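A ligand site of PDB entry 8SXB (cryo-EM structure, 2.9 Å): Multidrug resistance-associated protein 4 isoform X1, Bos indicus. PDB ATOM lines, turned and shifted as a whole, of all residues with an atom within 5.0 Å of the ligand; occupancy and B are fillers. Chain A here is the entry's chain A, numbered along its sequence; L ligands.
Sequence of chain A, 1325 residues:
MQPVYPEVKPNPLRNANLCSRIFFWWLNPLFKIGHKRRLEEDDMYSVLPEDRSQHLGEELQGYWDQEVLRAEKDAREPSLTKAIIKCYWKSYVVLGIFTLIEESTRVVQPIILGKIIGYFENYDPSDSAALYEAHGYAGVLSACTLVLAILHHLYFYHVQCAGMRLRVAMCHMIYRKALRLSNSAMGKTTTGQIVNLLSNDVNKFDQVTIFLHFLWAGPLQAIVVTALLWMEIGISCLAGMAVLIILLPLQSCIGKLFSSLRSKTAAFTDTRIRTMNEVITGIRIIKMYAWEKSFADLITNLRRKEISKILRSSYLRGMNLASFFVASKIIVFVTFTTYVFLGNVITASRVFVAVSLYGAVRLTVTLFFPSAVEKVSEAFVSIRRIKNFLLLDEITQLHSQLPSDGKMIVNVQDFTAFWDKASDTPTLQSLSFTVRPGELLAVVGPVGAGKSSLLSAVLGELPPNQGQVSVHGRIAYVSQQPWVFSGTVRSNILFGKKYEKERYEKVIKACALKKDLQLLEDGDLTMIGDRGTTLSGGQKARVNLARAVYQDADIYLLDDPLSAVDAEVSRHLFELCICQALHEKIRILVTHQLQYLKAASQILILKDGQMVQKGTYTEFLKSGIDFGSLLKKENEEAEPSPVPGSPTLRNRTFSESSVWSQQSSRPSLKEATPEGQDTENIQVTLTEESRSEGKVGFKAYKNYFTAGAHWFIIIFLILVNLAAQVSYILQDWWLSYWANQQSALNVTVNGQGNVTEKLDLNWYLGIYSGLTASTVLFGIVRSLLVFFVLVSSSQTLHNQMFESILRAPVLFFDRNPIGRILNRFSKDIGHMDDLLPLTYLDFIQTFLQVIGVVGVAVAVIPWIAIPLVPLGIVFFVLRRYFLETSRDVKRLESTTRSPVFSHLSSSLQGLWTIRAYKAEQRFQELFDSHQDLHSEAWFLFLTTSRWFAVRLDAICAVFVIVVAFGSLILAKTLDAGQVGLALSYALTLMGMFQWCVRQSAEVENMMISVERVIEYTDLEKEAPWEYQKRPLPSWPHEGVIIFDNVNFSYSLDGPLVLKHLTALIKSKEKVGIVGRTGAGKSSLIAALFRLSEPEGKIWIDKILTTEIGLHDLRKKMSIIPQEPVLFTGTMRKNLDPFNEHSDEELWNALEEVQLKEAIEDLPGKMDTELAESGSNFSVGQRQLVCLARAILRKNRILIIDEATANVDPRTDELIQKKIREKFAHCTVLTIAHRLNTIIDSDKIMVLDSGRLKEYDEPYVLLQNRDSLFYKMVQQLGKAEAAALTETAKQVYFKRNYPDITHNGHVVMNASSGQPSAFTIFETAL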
ATOM      1  N   HIS A 152      30.881  24.058  29.212  1.00  0.00           N
ATOM      2  CA  HIS A 152      30.569  23.100  28.162  1.00  0.00           C
ATOM      3  C   HIS A 152      31.491  23.244  26.964  1.00  0.00           C
ATOM      4  O   HIS A 152      31.988  22.249  26.436  1.00  0.00           O
ATOM      5  CB  HIS A 152      29.107  23.287  27.754  1.00  0.00           C
ATOM      6  CG  HIS A 152      28.662  22.469  26.570  1.00  0.00           C
ATOM      7  ND1 HIS A 152      28.920  22.828  25.263  1.00  0.00           N
ATOM      8  CD2 HIS A 152      27.943  21.335  26.501  1.00  0.00           C
ATOM      9  CE1 HIS A 152      28.395  21.937  24.450  1.00  0.00           C
ATOM     10  NE2 HIS A 152      27.800  21.011  25.183  1.00  0.00           N
ATOM     11  N   PHE A 156      34.317  20.278  25.880  1.00  0.00           N
ATOM     12  CA  PHE A 156      34.231  19.636  24.579  1.00  0.00           C
ATOM     13  C   PHE A 156      35.361  20.038  23.640  1.00  0.00           C
ATOM     14  O   PHE A 156      35.745  19.252  22.767  1.00  0.00           O
ATOM     15  CB  PHE A 156      32.857  19.914  23.965  1.00  0.00           C
ATOM     16  CG  PHE A 156      31.802  18.986  24.475  1.00  0.00           C
ATOM     17  CD1 PHE A 156      31.751  17.682  24.023  1.00  0.00           C
ATOM     18  CD2 PHE A 156      30.892  19.390  25.415  1.00  0.00           C
ATOM     19  CE1 PHE A 156      30.806  16.816  24.493  1.00  0.00           C
ATOM     20  CE2 PHE A 156      29.925  18.518  25.879  1.00  0.00           C
ATOM     21  CZ  PHE A 156      29.890  17.231  25.427  1.00  0.00           C
ATOM     22  N   GLN A 160      38.295  16.931  22.570  1.00  0.00           N
ATOM     23  CA  GLN A 160      38.465  16.704  21.148  1.00  0.00           C
ATOM     24  C   GLN A 160      39.910  16.888  20.700  1.00  0.00           C
ATOM     25  O   GLN A 160      40.347  16.238  19.749  1.00  0.00           O
ATOM     26  CB  GLN A 160      37.519  17.626  20.390  1.00  0.00           C
ATOM     27  CG  GLN A 160      36.082  17.138  20.471  1.00  0.00           C
ATOM     28  CD  GLN A 160      35.076  18.074  19.854  1.00  0.00           C
ATOM     29  OE1 GLN A 160      35.336  19.262  19.703  1.00  0.00           O
ATOM     30  NE2 GLN A 160      33.908  17.552  19.515  1.00  0.00           N
ATOM     31  N   PHE A 211      33.318  11.176  25.559  1.00  0.00           N
ATOM     32  CA  PHE A 211      32.271  10.901  26.548  1.00  0.00           C
ATOM     33  C   PHE A 211      32.734  10.169  27.805  1.00  0.00           C
ATOM     34  O   PHE A 211      31.892   9.912  28.669  1.00  0.00           O
ATOM     35  CB  PHE A 211      31.130  10.130  25.873  1.00  0.00           C
ATOM     36  CG  PHE A 211      30.535  10.828  24.694  1.00  0.00           C
ATOM     37  CD1 PHE A 211      29.660  11.881  24.870  1.00  0.00           C
ATOM     38  CD2 PHE A 211      30.847  10.447  23.404  1.00  0.00           C
ATOM     39  CE1 PHE A 211      29.108  12.539  23.801  1.00  0.00           C
ATOM     40  CE2 PHE A 211      30.292  11.100  22.313  1.00  0.00           C
ATOM     41  CZ  PHE A 211      29.425  12.159  22.524  1.00  0.00           C
ATOM     42  N   LEU A 321      18.606   6.175  19.668  1.00  0.00           N
ATOM     43  CA  LEU A 321      18.300   7.605  19.604  1.00  0.00           C
ATOM     44  C   LEU A 321      16.820   7.910  19.844  1.00  0.00           C
ATOM     45  O   LEU A 321      16.490   8.982  20.335  1.00  0.00           O
ATOM     46  CB  LEU A 321      18.761   8.147  18.257  1.00  0.00           C
ATOM     47  CG  LEU A 321      18.751   9.658  18.043  1.00  0.00           C
ATOM     48  CD1 LEU A 321      19.554  10.378  19.101  1.00  0.00           C
ATOM     49  CD2 LEU A 321      19.330   9.981  16.675  1.00  0.00           C
ATOM     50  N   PHE A 324      16.530   8.110  23.704  1.00  0.00           N
ATOM     51  CA  PHE A 324      16.854   9.445  24.209  1.00  0.00           C
ATOM     52  C   PHE A 324      15.706  10.422  24.033  1.00  0.00           C
ATOM     53  O   PHE A 324      15.430  11.232  24.925  1.00  0.00           O
ATOM     54  CB  PHE A 324      18.097   9.967  23.503  1.00  0.00           C
ATOM     55  CG  PHE A 324      18.337  11.438  23.711  1.00  0.00           C
ATOM     56  CD1 PHE A 324      18.574  11.946  24.982  1.00  0.00           C
ATOM     57  CD2 PHE A 324      18.300  12.315  22.644  1.00  0.00           C
ATOM     58  CE1 PHE A 324      18.787  13.300  25.168  1.00  0.00           C
ATOM     59  CE2 PHE A 324      18.513  13.669  22.830  1.00  0.00           C
ATOM     60  CZ  PHE A 324      18.754  14.162  24.086  1.00  0.00           C
ATOM     61  N   LEU A 363      20.458  13.936  29.552  1.00  0.00           N
ATOM     62  CA  LEU A 363      21.691  14.039  28.764  1.00  0.00           C
ATOM     63  C   LEU A 363      22.737  13.022  29.200  1.00  0.00           C
ATOM     64  O   LEU A 363      23.176  12.182  28.401  1.00  0.00           O
ATOM     65  CB  LEU A 363      22.277  15.443  28.863  1.00  0.00           C
ATOM     66  CG  LEU A 363      21.862  16.480  27.847  1.00  0.00           C
ATOM     67  CD1 LEU A 363      22.534  17.791  28.160  1.00  0.00           C
ATOM     68  CD2 LEU A 363      22.243  16.025  26.441  1.00  0.00           C
ATOM     69  N   LEU A 367      22.022   9.630  27.107  1.00  0.00           N
ATOM     70  CA  LEU A 367      22.723   9.920  25.851  1.00  0.00           C
ATOM     71  C   LEU A 367      24.230   9.759  25.996  1.00  0.00           C
ATOM     72  O   LEU A 367      24.823   8.987  25.238  1.00  0.00           O
ATOM     73  CB  LEU A 367      22.351  11.311  25.338  1.00  0.00           C
ATOM     74  CG  LEU A 367      22.966  11.761  24.002  1.00  0.00           C
ATOM     75  CD1 LEU A 367      22.481  10.920  22.846  1.00  0.00           C
ATOM     76  CD2 LEU A 367      22.631  13.202  23.732  1.00  0.00           C
ATOM     77  N   PHE A 368      24.883  10.484  26.918  1.00  0.00           N
ATOM     78  CA  PHE A 368      26.344  10.446  26.976  1.00  0.00           C
ATOM     79  C   PHE A 368      26.908   9.141  27.527  1.00  0.00           C
ATOM     80  O   PHE A 368      27.920   8.639  27.011  1.00  0.00           O
ATOM     81  CB  PHE A 368      26.878  11.621  27.809  1.00  0.00           C
ATOM     82  CG  PHE A 368      26.604  12.987  27.239  1.00  0.00           C
ATOM     83  CD1 PHE A 368      26.341  13.185  25.895  1.00  0.00           C
ATOM     84  CD2 PHE A 368      26.649  14.094  28.057  1.00  0.00           C
ATOM     85  CE1 PHE A 368      26.117  14.453  25.391  1.00  0.00           C
ATOM     86  CE2 PHE A 368      26.431  15.364  27.566  1.00  0.00           C
ATOM     87  CZ  PHE A 368      26.171  15.541  26.230  1.00  0.00           C
ATOM     88  N   LYS A 375      31.129   3.737  21.933  1.00  0.00           N
ATOM     89  CA  LYS A 375      32.382   4.206  21.330  1.00  0.00           C
ATOM     90  C   LYS A 375      33.616   3.572  21.982  1.00  0.00           C
ATOM     91  O   LYS A 375      34.644   3.437  21.311  1.00  0.00           O
ATOM     92  CB  LYS A 375      32.420   5.732  21.365  1.00  0.00           C
ATOM     93  CG  LYS A 375      31.528   6.257  20.268  1.00  0.00           C
ATOM     94  CD  LYS A 375      31.089   7.707  20.362  1.00  0.00           C
ATOM     95  CE  LYS A 375      30.284   8.011  19.109  1.00  0.00           C
ATOM     96  NZ  LYS A 375      29.881   9.435  18.933  1.00  0.00           N
ATOM     97  N   ASP A 842      19.219  12.865  13.400  1.00  0.00           N
ATOM     98  CA  ASP A 842      19.734  13.786  14.402  1.00  0.00           C
ATOM     99  C   ASP A 842      19.342  15.238  14.140  1.00  0.00           C
ATOM    100  O   ASP A 842      18.870  15.930  15.039  1.00  0.00           O
ATOM    101  CB  ASP A 842      21.259  13.622  14.430  1.00  0.00           C
ATOM    102  CG  ASP A 842      21.943  14.514  15.412  1.00  0.00           C
ATOM    103  OD1 ASP A 842      21.266  15.066  16.302  1.00  0.00           O
ATOM    104  OD2 ASP A 842      23.179  14.652  15.312  1.00  0.00           O
ATOM    105  N   GLN A 845      15.341  15.636  14.346  1.00  0.00           N
ATOM    106  CA  GLN A 845      14.876  15.548  15.723  1.00  0.00           C
ATOM    107  C   GLN A 845      15.221  16.794  16.540  1.00  0.00           C
ATOM    108  O   GLN A 845      14.395  17.241  17.336  1.00  0.00           O
ATOM    109  CB  GLN A 845      15.472  14.297  16.355  1.00  0.00           C
ATOM    110  CG  GLN A 845      15.108  14.054  17.805  1.00  0.00           C
ATOM    111  CD  GLN A 845      15.496  12.663  18.257  1.00  0.00           C
ATOM    112  OE1 GLN A 845      15.139  11.674  17.620  1.00  0.00           O
ATOM    113  NE2 GLN A 845      16.219  12.584  19.350  1.00  0.00           N
ATOM    114  N   THR A 846      16.416  17.372  16.371  1.00  0.00           N
ATOM    115  CA  THR A 846      16.720  18.625  17.080  1.00  0.00           C
ATOM    116  C   THR A 846      16.034  19.844  16.461  1.00  0.00           C
ATOM    117  O   THR A 846      15.520  20.682  17.200  1.00  0.00           O
ATOM    118  CB  THR A 846      18.227  18.872  17.126  1.00  0.00           C
ATOM    119  OG1 THR A 846      18.822  18.567  15.865  1.00  0.00           O
ATOM    120  CG2 THR A 846      18.888  18.061  18.202  1.00  0.00           C
ATOM    121  N   ARG A 946      34.197  26.082  17.413  1.00  0.00           N
ATOM    122  CA  ARG A 946      33.908  26.638  18.735  1.00  0.00           C
ATOM    123  C   ARG A 946      33.733  28.152  18.743  1.00  0.00           C
ATOM    124  O   ARG A 946      32.950  28.681  19.534  1.00  0.00           O
ATOM    125  CB  ARG A 946      35.014  26.252  19.722  1.00  0.00           C
ATOM    126  CG  ARG A 946      35.098  24.781  20.015  1.00  0.00           C
ATOM    127  CD  ARG A 946      33.908  24.250  20.799  1.00  0.00           C
ATOM    128  NE  ARG A 946      33.797  22.813  20.592  1.00  0.00           N
ATOM    129  CZ  ARG A 946      32.687  22.113  20.736  1.00  0.00           C
ATOM    130  NH1 ARG A 946      31.593  22.653  21.253  1.00  0.00           N
ATOM    131  NH2 ARG A 946      32.671  20.843  20.374  1.00  0.00           N
ATOM    132  N   GLY A 991      22.189  24.018  24.971  1.00  0.00           N
ATOM    133  CA  GLY A 991      22.979  22.997  24.300  1.00  0.00           C
ATOM    134  C   GLY A 991      22.507  22.716  22.891  1.00  0.00           C
ATOM    135  O   GLY A 991      23.302  22.468  21.986  1.00  0.00           O
ATOM    136  N   MET A 992      21.193  22.775  22.686  1.00  0.00           N
ATOM    137  CA  MET A 992      20.522  22.249  21.502  1.00  0.00           C
ATOM    138  C   MET A 992      20.743  23.100  20.245  1.00  0.00           C
ATOM    139  O   MET A 992      21.077  22.563  19.180  1.00  0.00           O
ATOM    140  CB  MET A 992      19.046  22.112  21.843  1.00  0.00           C
ATOM    141  CG  MET A 992      18.162  21.569  20.779  1.00  0.00           C
ATOM    142  SD  MET A 992      16.572  21.153  21.489  1.00  0.00           S
ATOM    143  CE  MET A 992      15.941  22.759  21.940  1.00  0.00           C
ATOM    144  N   GLN A 994      22.999  25.343  19.063  1.00  0.00           N
ATOM    145  CA  GLN A 994      24.287  25.266  18.363  1.00  0.00           C
ATOM    146  C   GLN A 994      24.519  23.917  17.681  1.00  0.00           C
ATOM    147  O   GLN A 994      25.118  23.865  16.608  1.00  0.00           O
ATOM    148  CB  GLN A 994      25.420  25.620  19.351  1.00  0.00           C
ATOM    149  CG  GLN A 994      25.681  24.644  20.491  1.00  0.00           C
ATOM    150  CD  GLN A 994      26.674  23.550  20.181  1.00  0.00           C
ATOM    151  OE1 GLN A 994      27.378  23.599  19.176  1.00  0.00           O
ATOM    152  NE2 GLN A 994      26.775  22.580  21.058  1.00  0.00           N
ATOM    153  N   TRP A 995      24.050  22.826  18.273  1.00  0.00           N
ATOM    154  CA  TRP A 995      24.202  21.516  17.638  1.00  0.00           C
ATOM    155  C   TRP A 995      23.337  21.409  16.394  1.00  0.00           C
ATOM    156  O   TRP A 995      23.785  20.926  15.351  1.00  0.00           O
ATOM    157  CB  TRP A 995      23.875  20.412  18.659  1.00  0.00           C
ATOM    158  CG  TRP A 995      24.112  19.014  18.167  1.00  0.00           C
ATOM    159  CD1 TRP A 995      23.157  18.090  17.854  1.00  0.00           C
ATOM    160  CD2 TRP A 995      25.372  18.370  17.930  1.00  0.00           C
ATOM    161  NE1 TRP A 995      23.738  16.926  17.454  1.00  0.00           N
ATOM    162  CE2 TRP A 995      25.092  17.076  17.471  1.00  0.00           C
ATOM    163  CE3 TRP A 995      26.696  18.782  18.040  1.00  0.00           C
ATOM    164  CZ2 TRP A 995      26.095  16.179  17.135  1.00  0.00           C
ATOM    165  CZ3 TRP A 995      27.693  17.879  17.715  1.00  0.00           C
ATOM    166  CH2 TRP A 995      27.389  16.595  17.266  1.00  0.00           C
ATOM    167  N   ARG A 998      25.071  23.436  13.570  1.00  0.00           N
ATOM    168  CA  ARG A 998      26.264  22.756  13.063  1.00  0.00           C
ATOM    169  C   ARG A 998      25.942  21.457  12.320  1.00  0.00           C
ATOM    170  O   ARG A 998      26.601  21.154  11.318  1.00  0.00           O
ATOM    171  CB  ARG A 998      27.246  22.528  14.205  1.00  0.00           C
ATOM    172  CG  ARG A 998      27.850  23.854  14.702  1.00  0.00           C
ATOM    173  CD  ARG A 998      29.114  23.711  15.530  1.00  0.00           C
ATOM    174  NE  ARG A 998      28.886  23.043  16.817  1.00  0.00           N
ATOM    175  CZ  ARG A 998      29.584  22.039  17.314  1.00  0.00           C
ATOM    176  NH1 ARG A 998      30.534  21.446  16.618  1.00  0.00           N
ATOM    177  NH2 ARG A 998      29.316  21.606  18.532  1.00  0.00           N
HETATM  178  C1  LIG L   1      28.399  18.827  21.811  1.00  0.00           C
HETATM  179  C2  LIG L   1      28.557  17.336  21.450  1.00  0.00           C
HETATM  180  C3  LIG L   1      27.510  16.459  22.169  1.00  0.00           C
HETATM  181  C4  LIG L   1      26.101  16.828  21.779  1.00  0.00           C
HETATM  182  C5  LIG L   1      25.370  17.751  22.396  1.00  0.00           C
HETATM  183  C6  LIG L   1      24.002  18.156  21.905  1.00  0.00           C
HETATM  184  C7  LIG L   1      22.882  17.820  22.902  1.00  0.00           C
HETATM  185  C8  LIG L   1      22.668  18.838  24.009  1.00  0.00           C
HETATM  186  O1  LIG L   1      23.547  19.373  24.655  1.00  0.00           O
HETATM  187  C9  LIG L   1      21.510  17.711  22.220  1.00  0.00           C
HETATM  188  C10 LIG L   1      20.547  17.974  23.386  1.00  0.00           C
HETATM  189  O2  LIG L   1      19.248  18.287  22.921  1.00  0.00           O
HETATM  190  C11 LIG L   1      21.189  19.097  24.199  1.00  0.00           C
HETATM  191  C12 LIG L   1      21.294  16.341  21.632  1.00  0.00           C
HETATM  192  C13 LIG L   1      20.890  16.072  20.402  1.00  0.00           C
HETATM  193  C14 LIG L   1      20.896  14.687  19.833  1.00  0.00           C
HETATM  194  O3  LIG L   1      20.126  14.658  18.639  1.00  0.00           O
HETATM  195  C15 LIG L   1      22.346  14.294  19.592  1.00  0.00           C
HETATM  196  C16 LIG L   1      22.568  12.871  19.070  1.00  0.00           C
HETATM  197  C17 LIG L   1      24.051  12.605  18.692  1.00  0.00           C
HETATM  198  C18 LIG L   1      25.065  13.025  19.782  1.00  0.00           C
HETATM  199  C19 LIG L   1      26.487  12.580  19.427  1.00  0.00           C
HETATM  200  O4  LIG L   1      29.250  20.946  21.365  1.00  0.00           O
HETATM  201  C20 LIG L   1      29.405  19.769  21.166  1.00  0.00           C
HETATM  202  O5  LIG L   1      30.307  19.336  20.482  1.00  0.00           O
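NH2 of Arg 998 is in salt-bridge range of O4 of the ligand (2.9 Å). An oxygen (O5) of the ligand lies within salt-bridge range of the guanidinium group of Arg 946, 2.8 Å away. The side-chain carboxylate of Asp 842 sits at hydrogen-bond distance from an oxygen (O3) of the ligand (2.6 Å). NE2 of Gln 994 is in hydrogen-bond range of O4 of the ligand (3.0 Å).
NH2 of Arg 998 is in hydrogen-bond range of OE1 of Gln 994 (2.9 Å). The side-chain amide oxygen (OE1) of Gln 160 sits close to the backbone carbonyl oxygen (O) of Phe 156 (3.1 Å). The indole nitrogen of Trp 995 sits at hydrogen-bond distance from the side-chain carboxylate of Asp 842. The guanidinium group (NH2) of Arg 946 is in hydrogen-bond range of the side-chain amide oxygen (OE1) of Gln 160 (3.2 Å). O of Leu 363 is in hydrogen-bond range of N of Phe 368 (2.8 Å). O of Asp 842 lies within hydrogen-bond range of OG1 of Thr 846 (2.8 Å).
Residues that only touch the ligand: His 152 (3.4 Å), Phe 156 (3.8 Å), Leu 321 (3.9 Å), Phe 324 (3.96 Å), Leu 363 (3.7 Å), Thr 846 (3.6 Å), Gly 991 (3.7 Å), Met 992 (3.98 Å) and Trp 995 (3.7 Å). Hydrophobic or aromatic side chains that line the ligand: His 152, Phe 156, Leu 321, Phe 324, Leu 363, Met 992 and Trp 995. Of the 19 residues printed, 13 come within 4 Å of the ligand. Along chain A the residues within 4 Å of the ligand span positions 152 to 998.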
